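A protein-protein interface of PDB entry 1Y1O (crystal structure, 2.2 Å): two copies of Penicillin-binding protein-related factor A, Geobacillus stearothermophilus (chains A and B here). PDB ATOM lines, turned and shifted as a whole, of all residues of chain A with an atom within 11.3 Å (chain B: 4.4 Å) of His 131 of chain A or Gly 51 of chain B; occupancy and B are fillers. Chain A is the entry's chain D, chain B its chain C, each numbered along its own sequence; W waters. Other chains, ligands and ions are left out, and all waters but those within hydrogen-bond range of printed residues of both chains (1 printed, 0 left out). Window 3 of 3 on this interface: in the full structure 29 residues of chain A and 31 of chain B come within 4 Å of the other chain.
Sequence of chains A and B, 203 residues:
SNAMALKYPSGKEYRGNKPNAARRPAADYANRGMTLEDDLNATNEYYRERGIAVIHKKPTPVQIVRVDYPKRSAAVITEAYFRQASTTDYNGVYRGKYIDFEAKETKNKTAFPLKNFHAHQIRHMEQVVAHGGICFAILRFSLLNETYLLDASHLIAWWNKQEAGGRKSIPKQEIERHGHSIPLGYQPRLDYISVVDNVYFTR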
ATOM      1  N   GLY A  96      14.669   3.175  11.294  1.00  0.00           N
ATOM      2  CA  GLY A  96      13.816   3.111  12.502  1.00  0.00           C
ATOM      3  C   GLY A  96      14.499   2.917  13.858  1.00  0.00           C
ATOM      4  O   GLY A  96      13.831   2.907  14.888  1.00  0.00           O
ATOM      5  N   LYS A  97      15.820   2.771  13.856  1.00  0.00           N
ATOM      6  CA  LYS A  97      16.597   2.479  15.046  1.00  0.00           C
ATOM      7  C   LYS A  97      17.311   3.707  15.534  1.00  0.00           C
ATOM      8  O   LYS A  97      17.642   4.615  14.786  1.00  0.00           O
ATOM      9  CB  LYS A  97      17.632   1.367  14.773  1.00  0.00           C
ATOM     10  CG  LYS A  97      17.017   0.025  14.310  1.00  0.00           C
ATOM     11  CD  LYS A  97      16.298  -0.647  15.432  1.00  0.00           C
ATOM     12  CE  LYS A  97      16.137  -2.133  15.140  1.00  0.00           C
ATOM     13  NZ  LYS A  97      15.224  -2.747  16.141  1.00  0.00           N
ATOM     14  N   TYR A  98      17.547   3.730  16.832  1.00  0.00           N
ATOM     15  CA  TYR A  98      18.287   4.800  17.420  1.00  0.00           C
ATOM     16  C   TYR A  98      19.764   4.428  17.330  1.00  0.00           C
ATOM     17  O   TYR A  98      20.156   3.344  17.743  1.00  0.00           O
ATOM     18  CB  TYR A  98      17.825   4.974  18.865  1.00  0.00           C
ATOM     19  CG  TYR A  98      18.652   5.910  19.672  1.00  0.00           C
ATOM     20  CD1 TYR A  98      18.452   7.290  19.591  1.00  0.00           C
ATOM     21  CD2 TYR A  98      19.660   5.420  20.548  1.00  0.00           C
ATOM     22  CE1 TYR A  98      19.215   8.175  20.372  1.00  0.00           C
ATOM     23  CE2 TYR A  98      20.419   6.310  21.311  1.00  0.00           C
ATOM     24  CZ  TYR A  98      20.208   7.675  21.208  1.00  0.00           C
ATOM     25  OH  TYR A  98      20.948   8.556  21.988  1.00  0.00           O
ATOM     26  N   ILE A  99      20.549   5.312  16.738  1.00  0.00           N
ATOM     27  CA  ILE A  99      21.984   5.139  16.589  1.00  0.00           C
ATOM     28  C   ILE A  99      22.652   6.153  17.508  1.00  0.00           C
ATOM     29  O   ILE A  99      22.241   7.314  17.576  1.00  0.00           O
ATOM     30  CB  ILE A  99      22.486   5.451  15.148  1.00  0.00           C
ATOM     31  CG1 ILE A  99      21.673   4.758  14.054  1.00  0.00           C
ATOM     32  CG2 ILE A  99      24.008   5.143  15.003  1.00  0.00           C
ATOM     33  CD1 ILE A  99      21.177   3.331  14.371  1.00  0.00           C
ATOM     34  N   ASP A 100      23.690   5.732  18.188  1.00  0.00           N
ATOM     35  CA  ASP A 100      24.316   6.563  19.215  1.00  0.00           C
ATOM     36  C   ASP A 100      25.790   6.160  19.269  1.00  0.00           C
ATOM     37  O   ASP A 100      26.117   4.977  19.365  1.00  0.00           O
ATOM     38  CB  ASP A 100      23.563   6.356  20.541  1.00  0.00           C
ATOM     39  CG  ASP A 100      24.134   7.154  21.707  1.00  0.00           C
ATOM     40  OD1 ASP A 100      25.330   7.006  22.011  1.00  0.00           O
ATOM     41  OD2 ASP A 100      23.374   7.871  22.393  1.00  0.00           O
ATOM     42  N   ILE A 122      29.903   6.255  29.505  1.00  0.00           N
ATOM     43  CA  ILE A 122      29.867   4.803  29.577  1.00  0.00           C
ATOM     44  C   ILE A 122      28.515   4.323  30.144  1.00  0.00           C
ATOM     45  O   ILE A 122      27.986   3.303  29.706  1.00  0.00           O
ATOM     46  CB  ILE A 122      31.066   4.210  30.407  1.00  0.00           C
ATOM     47  CG1 ILE A 122      32.424   4.494  29.722  1.00  0.00           C
ATOM     48  CG2 ILE A 122      30.883   2.697  30.673  1.00  0.00           C
ATOM     49  CD1 ILE A 122      32.559   3.956  28.301  1.00  0.00           C
ATOM     50  N   ARG A 123      27.959   5.065  31.104  1.00  0.00           N
ATOM     51  CA  ARG A 123      26.728   4.639  31.765  1.00  0.00           C
ATOM     52  C   ARG A 123      25.551   4.921  30.864  1.00  0.00           C
ATOM     53  O   ARG A 123      24.593   4.172  30.881  1.00  0.00           O
ATOM     54  CB  ARG A 123      26.511   5.347  33.104  1.00  0.00           C
ATOM     55  CG  ARG A 123      27.543   4.997  34.198  1.00  0.00           C
ATOM     56  CD  ARG A 123      27.828   3.491  34.199  1.00  0.00           C
ATOM     57  NE  ARG A 123      29.219   3.205  34.562  1.00  0.00           N
ATOM     58  CZ  ARG A 123      29.767   1.995  34.544  1.00  0.00           C
ATOM     59  NH1 ARG A 123      29.052   0.952  34.165  1.00  0.00           N
ATOM     60  NH2 ARG A 123      31.034   1.822  34.907  1.00  0.00           N
ATOM     61  N   HIS A 124      25.633   6.022  30.113  1.00  0.00           N
ATOM     62  CA  HIS A 124      24.623   6.372  29.115  1.00  0.00           C
ATOM     63  C   HIS A 124      24.494   5.258  28.057  1.00  0.00           C
ATOM     64  O   HIS A 124      23.376   4.818  27.765  1.00  0.00           O
ATOM     65  CB  HIS A 124      24.935   7.718  28.449  1.00  0.00           C
ATOM     66  CG  HIS A 124      24.158   7.953  27.184  1.00  0.00           C
ATOM     67  ND1 HIS A 124      22.820   8.291  27.180  1.00  0.00           N
ATOM     68  CD2 HIS A 124      24.522   7.856  25.886  1.00  0.00           C
ATOM     69  CE1 HIS A 124      22.402   8.419  25.933  1.00  0.00           C
ATOM     70  NE2 HIS A 124      23.417   8.164  25.129  1.00  0.00           N
ATOM     71  N   MET A 125      25.636   4.808  27.529  1.00  0.00           N
ATOM     72  CA  MET A 125      25.729   3.718  26.555  1.00  0.00           C
ATOM     73  C   MET A 125      25.088   2.419  27.040  1.00  0.00           C
ATOM     74  O   MET A 125      24.417   1.728  26.249  1.00  0.00           O
ATOM     75  CB  MET A 125      27.189   3.446  26.154  1.00  0.00           C
ATOM     76  CG  MET A 125      27.800   4.561  25.343  1.00  0.00           C
ATOM     77  SD  MET A 125      29.762   4.455  24.983  1.00  0.00           S
ATOM     78  CE  MET A 125      29.717   3.734  23.085  1.00  0.00           C
ATOM     79  N   GLU A 126      25.319   2.081  28.321  1.00  0.00           N
ATOM     80  CA  GLU A 126      24.739   0.897  28.952  1.00  0.00           C
ATOM     81  C   GLU A 126      23.220   0.984  28.885  1.00  0.00           C
ATOM     82  O   GLU A 126      22.532   0.026  28.589  1.00  0.00           O
ATOM     83  CB  GLU A 126      25.179   0.767  30.440  1.00  0.00           C
ATOM     84  CG  GLU A 126      26.601   0.277  30.644  1.00  0.00           C
ATOM     85  CD  GLU A 126      27.054   0.190  32.124  1.00  0.00           C
ATOM     86  OE1 GLU A 126      26.285   0.494  33.074  1.00  0.00           O
ATOM     87  OE2 GLU A 126      28.219  -0.201  32.347  1.00  0.00           O
ATOM     88  N   GLN A 127      22.708   2.161  29.178  1.00  0.00           N
ATOM     89  CA  GLN A 127      21.278   2.389  29.118  1.00  0.00           C
ATOM     90  C   GLN A 127      20.714   2.294  27.695  1.00  0.00           C
ATOM     91  O   GLN A 127      19.603   1.780  27.491  1.00  0.00           O
ATOM     92  CB  GLN A 127      20.961   3.739  29.734  1.00  0.00           C
ATOM     93  CG  GLN A 127      21.167   3.810  31.273  1.00  0.00           C
ATOM     94  CD  GLN A 127      20.765   5.208  31.822  1.00  0.00           C
ATOM     95  OE1 GLN A 127      20.365   5.338  32.987  1.00  0.00           O
ATOM     96  NE2 GLN A 127      20.843   6.251  30.964  1.00  0.00           N
ATOM     97  N   VAL A 128      21.486   2.733  26.720  1.00  0.00           N
ATOM     98  CA  VAL A 128      21.052   2.689  25.330  1.00  0.00           C
ATOM     99  C   VAL A 128      21.023   1.274  24.796  1.00  0.00           C
ATOM    100  O   VAL A 128      20.059   0.896  24.106  1.00  0.00           O
ATOM    101  CB  VAL A 128      21.862   3.659  24.414  1.00  0.00           C
ATOM    102  CG1 VAL A 128      21.584   3.385  22.909  1.00  0.00           C
ATOM    103  CG2 VAL A 128      21.577   5.143  24.786  1.00  0.00           C
ATOM    104  N   VAL A 129      22.035   0.484  25.142  1.00  0.00           N
ATOM    105  CA  VAL A 129      22.110  -0.893  24.668  1.00  0.00           C
ATOM    106  C   VAL A 129      20.963  -1.682  25.288  1.00  0.00           C
ATOM    107  O   VAL A 129      20.263  -2.407  24.595  1.00  0.00           O
ATOM    108  CB  VAL A 129      23.459  -1.597  25.033  1.00  0.00           C
ATOM    109  CG1 VAL A 129      23.408  -3.083  24.624  1.00  0.00           C
ATOM    110  CG2 VAL A 129      24.656  -0.878  24.384  1.00  0.00           C
ATOM    111  N   ALA A 130      20.816  -1.556  26.605  1.00  0.00           N
ATOM    112  CA  ALA A 130      19.707  -2.176  27.333  1.00  0.00           C
ATOM    113  C   ALA A 130      18.341  -1.871  26.722  1.00  0.00           C
ATOM    114  O   ALA A 130      17.466  -2.721  26.772  1.00  0.00           O
ATOM    115  CB  ALA A 130      19.738  -1.785  28.826  1.00  0.00           C
ATOM    116  N   HIS A 131      18.154  -0.685  26.117  1.00  0.00           N
ATOM    117  CA  HIS A 131      16.832  -0.345  25.595  1.00  0.00           C
ATOM    118  C   HIS A 131      16.669  -0.637  24.116  1.00  0.00           C
ATOM    119  O   HIS A 131      15.668  -0.249  23.514  1.00  0.00           O
ATOM    120  CB  HIS A 131      16.432   1.096  25.921  1.00  0.00           C
ATOM    121  CG  HIS A 131      15.908   1.262  27.315  1.00  0.00           C
ATOM    122  ND1 HIS A 131      16.730   1.482  28.401  1.00  0.00           N
ATOM    123  CD2 HIS A 131      14.648   1.201  27.806  1.00  0.00           C
ATOM    124  CE1 HIS A 131      15.996   1.565  29.496  1.00  0.00           C
ATOM    125  NE2 HIS A 131      14.730   1.404  29.160  1.00  0.00           N
ATOM    126  N   GLY A 132      17.647  -1.306  23.522  1.00  0.00           N
ATOM    127  CA  GLY A 132      17.526  -1.695  22.125  1.00  0.00           C
ATOM    128  C   GLY A 132      18.120  -0.712  21.136  1.00  0.00           C
ATOM    129  O   GLY A 132      17.931  -0.875  19.945  1.00  0.00           O
ATOM    130  N   GLY A 133      18.845   0.298  21.621  1.00  0.00           N
ATOM    131  CA  GLY A 133      19.602   1.178  20.748  1.00  0.00           C
ATOM    132  C   GLY A 133      20.810   0.535  20.062  1.00  0.00           C
ATOM    133  O   GLY A 133      21.336  -0.490  20.508  1.00  0.00           O
ATOM    134  N   ILE A 134      21.283   1.162  18.987  1.00  0.00           N
ATOM    135  CA  ILE A 134      22.517   0.735  18.366  1.00  0.00           C
ATOM    136  C   ILE A 134      23.583   1.700  18.784  1.00  0.00           C
ATOM    137  O   ILE A 134      23.553   2.908  18.422  1.00  0.00           O
ATOM    138  CB  ILE A 134      22.430   0.690  16.834  1.00  0.00           C
ATOM    139  CG1 ILE A 134      21.365  -0.350  16.400  1.00  0.00           C
ATOM    140  CG2 ILE A 134      23.829   0.440  16.250  1.00  0.00           C
ATOM    141  CD1 ILE A 134      21.084  -0.318  14.924  1.00  0.00           C
ATOM    142  N   CYS A 135      24.521   1.169  19.562  1.00  0.00           N
ATOM    143  CA  CYS A 135      25.465   2.018  20.285  1.00  0.00           C
ATOM    144  C   CYS A 135      26.928   1.541  20.115  1.00  0.00           C
ATOM    145  O   CYS A 135      27.239   0.393  20.377  1.00  0.00           O
ATOM    146  CB  CYS A 135      25.015   2.104  21.750  1.00  0.00           C
ATOM    147  SG  CYS A 135      25.912   3.313  22.720  1.00  0.00           S
ATOM    148  N   ASP A 151      31.410  -2.168  19.104  1.00  0.00           N
ATOM    149  CA  ASP A 151      30.202  -2.193  19.884  1.00  0.00           C
ATOM    150  C   ASP A 151      30.409  -1.765  21.325  1.00  0.00           C
ATOM    151  O   ASP A 151      31.423  -2.115  21.953  1.00  0.00           O
ATOM    152  CB  ASP A 151      29.523  -3.563  19.839  1.00  0.00           C
ATOM    153  CG  ASP A 151      28.093  -3.484  20.287  1.00  0.00           C
ATOM    154  OD1 ASP A 151      27.268  -2.899  19.538  1.00  0.00           O
ATOM    155  OD2 ASP A 151      27.800  -3.943  21.416  1.00  0.00           O
ATOM    156  N   ALA A 152      29.420  -1.025  21.846  1.00  0.00           N
ATOM    157  CA  ALA A 152      29.485  -0.393  23.163  1.00  0.00           C
ATOM    158  C   ALA A 152      29.728  -1.385  24.268  1.00  0.00           C
ATOM    159  O   ALA A 152      30.256  -0.994  25.314  1.00  0.00           O
ATOM    160  CB  ALA A 152      28.196   0.412  23.477  1.00  0.00           C
ATOM    161  N   ILE A 156      32.190  -0.908  27.210  1.00  0.00           N
ATOM    162  CA  ILE A 156      31.669  -0.910  28.586  1.00  0.00           C
ATOM    163  C   ILE A 156      32.477  -1.895  29.460  1.00  0.00           C
ATOM    164  O   ILE A 156      32.910  -1.559  30.588  1.00  0.00           O
ATOM    165  CB  ILE A 156      30.156  -1.309  28.609  1.00  0.00           C
ATOM    166  CG1 ILE A 156      29.267  -0.172  28.033  1.00  0.00           C
ATOM    167  CG2 ILE A 156      29.724  -1.755  30.021  1.00  0.00           C
ATOM    168  CD1 ILE A 156      27.898  -0.638  27.408  1.00  0.00           C
ATOM    169  N   TYR B  47      11.938   8.298  33.860  1.00  0.00           N
ATOM    170  CA  TYR B  47      12.058   7.165  32.899  1.00  0.00           C
ATOM    171  C   TYR B  47      13.471   6.510  32.852  1.00  0.00           C
ATOM    172  O   TYR B  47      13.618   5.280  32.811  1.00  0.00           O
ATOM    173  CB  TYR B  47      11.637   7.581  31.483  1.00  0.00           C
ATOM    174  CG  TYR B  47      10.169   7.975  31.286  1.00  0.00           C
ATOM    175  CD1 TYR B  47       9.113   7.250  31.876  1.00  0.00           C
ATOM    176  CD2 TYR B  47       9.837   9.039  30.453  1.00  0.00           C
ATOM    177  CE1 TYR B  47       7.804   7.602  31.658  1.00  0.00           C
ATOM    178  CE2 TYR B  47       8.538   9.396  30.238  1.00  0.00           C
ATOM    179  CZ  TYR B  47       7.515   8.688  30.828  1.00  0.00           C
ATOM    180  OH  TYR B  47       6.211   9.081  30.578  1.00  0.00           O
ATOM    181  N   ARG B  48      14.503   7.330  32.847  1.00  0.00           N
ATOM    182  CA  ARG B  48      15.870   6.818  32.876  1.00  0.00           C
ATOM    183  C   ARG B  48      16.168   6.017  34.138  1.00  0.00           C
ATOM    184  O   ARG B  48      16.661   4.889  34.056  1.00  0.00           O
ATOM    185  CB  ARG B  48      16.889   7.946  32.682  1.00  0.00           C
ATOM    186  CG  ARG B  48      17.040   8.386  31.224  1.00  0.00           C
ATOM    187  CD  ARG B  48      18.200   9.369  30.995  1.00  0.00           C
ATOM    188  NE  ARG B  48      18.313  10.401  32.028  1.00  0.00           N
ATOM    189  CZ  ARG B  48      17.790  11.633  31.967  1.00  0.00           C
ATOM    190  NH1 ARG B  48      17.089  12.064  30.919  1.00  0.00           N
ATOM    191  NH2 ARG B  48      17.991  12.456  32.978  1.00  0.00           N
ATOM    192  N   GLU B  49      15.838   6.590  35.296  1.00  0.00           N
ATOM    193  CA  GLU B  49      16.057   5.932  36.593  1.00  0.00           C
ATOM    194  C   GLU B  49      15.324   4.618  36.681  1.00  0.00           C
ATOM    195  O   GLU B  49      15.862   3.653  37.204  1.00  0.00           O
ATOM    196  CB  GLU B  49      15.602   6.816  37.758  1.00  0.00           C
ATOM    197  CG  GLU B  49      16.412   8.095  37.921  1.00  0.00           C
ATOM    198  CD  GLU B  49      15.788   9.067  38.930  1.00  0.00           C
ATOM    199  OE1 GLU B  49      14.547   9.014  39.179  1.00  0.00           O
ATOM    200  OE2 GLU B  49      16.556   9.899  39.472  1.00  0.00           O
ATOM    201  N   ARG B  50      14.108   4.571  36.152  1.00  0.00           N
ATOM    202  CA  ARG B  50      13.274   3.385  36.294  1.00  0.00           C
ATOM    203  C   ARG B  50      13.558   2.289  35.259  1.00  0.00           C
ATOM    204  O   ARG B  50      12.970   1.209  35.319  1.00  0.00           O
ATOM    205  CB  ARG B  50      11.791   3.777  36.335  1.00  0.00           C
ATOM    206  CG  ARG B  50      11.389   4.625  37.571  1.00  0.00           C
ATOM    207  CD  ARG B  50      11.459   3.861  38.919  1.00  0.00           C
ATOM    208  NE  ARG B  50      10.682   2.614  38.936  1.00  0.00           N
ATOM    209  CZ  ARG B  50       9.478   2.461  39.505  1.00  0.00           C
ATOM    210  NH1 ARG B  50       8.879   3.478  40.122  1.00  0.00           N
ATOM    211  NH2 ARG B  50       8.859   1.283  39.461  1.00  0.00           N
ATOM    212  N   GLY B  51      14.488   2.547  34.349  1.00  0.00           N
ATOM    213  CA  GLY B  51      14.745   1.651  33.222  1.00  0.00           C
ATOM    214  C   GLY B  51      13.602   1.573  32.213  1.00  0.00           C
ATOM    215  O   GLY B  51      13.404   0.544  31.589  1.00  0.00           O
ATOM    216  N   ILE B  52      12.873   2.673  32.022  1.00  0.00           N
ATOM    217  CA  ILE B  52      11.721   2.710  31.112  1.00  0.00           C
ATOM    218  C   ILE B  52      12.102   3.127  29.670  1.00  0.00           C
ATOM    219  O   ILE B  52      11.758   2.438  28.697  1.00  0.00           O
ATOM    220  CB  ILE B  52      10.576   3.589  31.702  1.00  0.00           C
ATOM    221  CG1 ILE B  52      10.070   2.963  33.016  1.00  0.00           C
ATOM    222  CG2 ILE B  52       9.426   3.811  30.681  1.00  0.00           C
ATOM    223  CD1 ILE B  52       9.111   3.869  33.877  1.00  0.00           C
ATOM    224  N   ALA B  53      12.844   4.223  29.567  1.00  0.00           N
ATOM    225  CA  ALA B  53      13.207   4.875  28.304  1.00  0.00           C
ATOM    226  C   ALA B  53      14.448   5.704  28.525  1.00  0.00           C
ATOM    227  O   ALA B  53      14.633   6.236  29.622  1.00  0.00           O
ATOM    228  CB  ALA B  53      12.062   5.786  27.809  1.00  0.00           C
ATOM    229  N   VAL B  54      15.273   5.849  27.491  1.00  0.00           N
ATOM    230  CA  VAL B  54      16.452   6.735  27.555  1.00  0.00           C
ATOM    231  C   VAL B  54      16.219   7.912  26.620  1.00  0.00           C
ATOM    232  O   VAL B  54      16.432   7.804  25.421  1.00  0.00           O
ATOM    233  CB  VAL B  54      17.796   6.039  27.131  1.00  0.00           C
ATOM    234  CG1 VAL B  54      19.040   6.893  27.591  1.00  0.00           C
ATOM    235  CG2 VAL B  54      17.915   4.625  27.692  1.00  0.00           C
ATOM    236  N   VAL B  93      15.704   6.530  22.854  1.00  0.00           N
ATOM    237  CA  VAL B  93      15.285   5.211  22.454  1.00  0.00           C
ATOM    238  C   VAL B  93      14.295   4.657  23.493  1.00  0.00           C
ATOM    239  O   VAL B  93      14.482   4.820  24.712  1.00  0.00           O
ATOM    240  CB  VAL B  93      16.480   4.228  22.214  1.00  0.00           C
ATOM    241  CG1 VAL B  93      17.430   4.132  23.450  1.00  0.00           C
ATOM    242  CG2 VAL B  93      15.952   2.826  21.808  1.00  0.00           C
ATOM    243  N   ARG B  95      11.878   0.907  23.711  1.00  0.00           N
ATOM    244  CA  ARG B  95      11.500  -0.417  23.177  1.00  0.00           C
ATOM    245  C   ARG B  95      12.080  -0.724  21.797  1.00  0.00           C
ATOM    246  O   ARG B  95      11.363  -1.260  20.938  1.00  0.00           O
ATOM    247  CB  ARG B  95       9.963  -0.582  23.157  1.00  0.00           C
ATOM    248  CG  ARG B  95       9.322  -0.631  24.558  1.00  0.00           C
ATOM    249  CD  ARG B  95       7.792  -0.615  24.509  1.00  0.00           C
ATOM    250  NE  ARG B  95       7.229  -1.837  23.937  1.00  0.00           N
ATOM    251  CZ  ARG B  95       5.941  -2.014  23.661  1.00  0.00           C
ATOM    252  NH1 ARG B  95       5.044  -1.065  23.913  1.00  0.00           N
ATOM    253  NH2 ARG B  95       5.546  -3.160  23.133  1.00  0.00           N
ATOM    254  N   GLY B  96      13.338  -0.340  21.575  1.00  0.00           N
ATOM    255  CA  GLY B  96      14.012  -0.537  20.286  1.00  0.00           C
ATOM    256  C   GLY B  96      13.778   0.509  19.196  1.00  0.00           C
ATOM    257  O   GLY B  96      14.341   0.417  18.100  1.00  0.00           O
HETATM  258  O   HOH W   1      16.859   1.215  18.349  1.00  0.00           O
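Printed residues of chain A that touch a printed residue of chain B: Lys 97, Tyr 98, Gln 127, His 131, Gly 132 and Gly 133.
Hydrophobic or aromatic side chains of chain A within 4 Å of the printed part of chain B: Tyr 98 and His 131.
Along chain A the printed residues that touch a printed residue of chain B span positions 97 to 133.
Of the 11 printed residues of chain B, 8 touch a printed residue of chain A.
Along chain B the printed residues that touch a printed residue of chain A span positions 48 to 96.
Among the printed residues, 13 pairs touch across the chains.
Position printed for both chains: 96.
Of the 13 pairs that touch across the chains among the printed residues, none has its exchanged pair printed and touching as well.
Gly 96 of chain B touches Lys 97 of chain A.
CB of Val 93 of chain B touches CB of Tyr 98 of chain A, at 3.7 Å.
Gln 127 of chain A touches Arg 48 of chain B.
Gln 127 of chain A touches Val 54 of chain B.
Val 54 of chain B touches His 131 of chain A.
His 131 of chain A touches Val 93 of chain B (O to CG2, 3.5 Å).
His 131 of chain A touches Arg 95 of chain B.
Gly 96 of chain B touches Gly 132 of chain A (CA to O, 3.9 Å).
Gly 133 of chain A touches Val 93 of chain B (N to CG2, 3.8 Å).
The backbone NH (N) of Gly 96 of chain B sits at hydrogen-bond distance from the backbone carbonyl oxygen (O) of His 131 of chain A, at 3.0 Å.
The backbone NH (N) of Ala 53 of chain B is in hydrogen-bond range of a ring nitrogen (NE2) of His 131 of chain A, at 3.4 Å.
The backbone carbonyl oxygen (O) of Gly 51 of chain B sits at hydrogen-bond distance from a ring nitrogen (NE2) of His 131 of chain A (2.9 Å).
O of Ile 52 of chain B lies within hydrogen-bond range of NE2 of His 131 of chain A (3.2 Å).
The backbone NH (N) of Ile 134 of chain A lies within hydrogen-bond range of the backbone carbonyl oxygen (O) of Tyr 98 of chain A (2.8 Å).
The side-chain hydroxyl of Tyr 98 of chain A is in hydrogen-bond range of the side-chain carboxylate of Asp 100 of chain A.
The backbone NH (N) of Val 93 of chain B lies within hydrogen-bond range of the backbone carbonyl oxygen (O) of Val 54 of chain B, at 3.0 Å.
The backbone NH (N) of Arg 48 of chain B lies within hydrogen-bond range of the backbone carbonyl oxygen (O) of Ala 53 of chain B (3.4 Å).
N of Ala 53 of chain B lies within hydrogen-bond range of O of Tyr 47 of chain B.
The backbone carbonyl oxygen (O) of Gln 127 of chain A is in hydrogen-bond range of a ring nitrogen (ND1) of His 131 of chain A (3.0 Å).
Printed residues of chain B within 4 Å of Lys 97 of chain A: Gly 96 (3.5 Å).
Arg 123 of chain A touches none of the printed residues of chain B.
Of chain B, only Gly 51 (2.9 Å), Ile 52 (3.2 Å), Ala 53 (3.4 Å), Val 54 (3.4 Å), Val 93 (3.5 Å), Arg 95 (3.97 Å) and Gly 96 (3.0 Å) come within 4 Å of His 131 of chain A.
Of the printed residues of chain B, Gly 132 of chain A touches Gly 96 (3.9 Å).
Cys 135 of chain A touches none of the printed residues of chain B.
Of the printed residues of chain A, Arg 48 of chain B touches Gln 127 (3.9 Å).
Gly 51 of chain B touches one residue of chain A.
Printed residues of chain A within 4 Å of Ile 52 of chain B: His 131 (3.2 Å).
Val 54 of chain B touches just these residues of chain A: Gln 127 and His 131.
Printed residues of chain A within 4 Å of Gly 96 of chain B: Lys 97, His 131 and Gly 132.
The nearest printed residue of chain B that does not touch His 131 of chain A is Tyr 47 of chain B (5.4 Å).
The nearest printed residue of chain B that does not touch Tyr 98 of chain A is Gly 96 of chain B (4.8 Å).
Water W1 lies within hydrogen-bond range of O of Gly 96 of chain B, O of Gly 132 of chain A and N of Tyr 98 of chain A.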
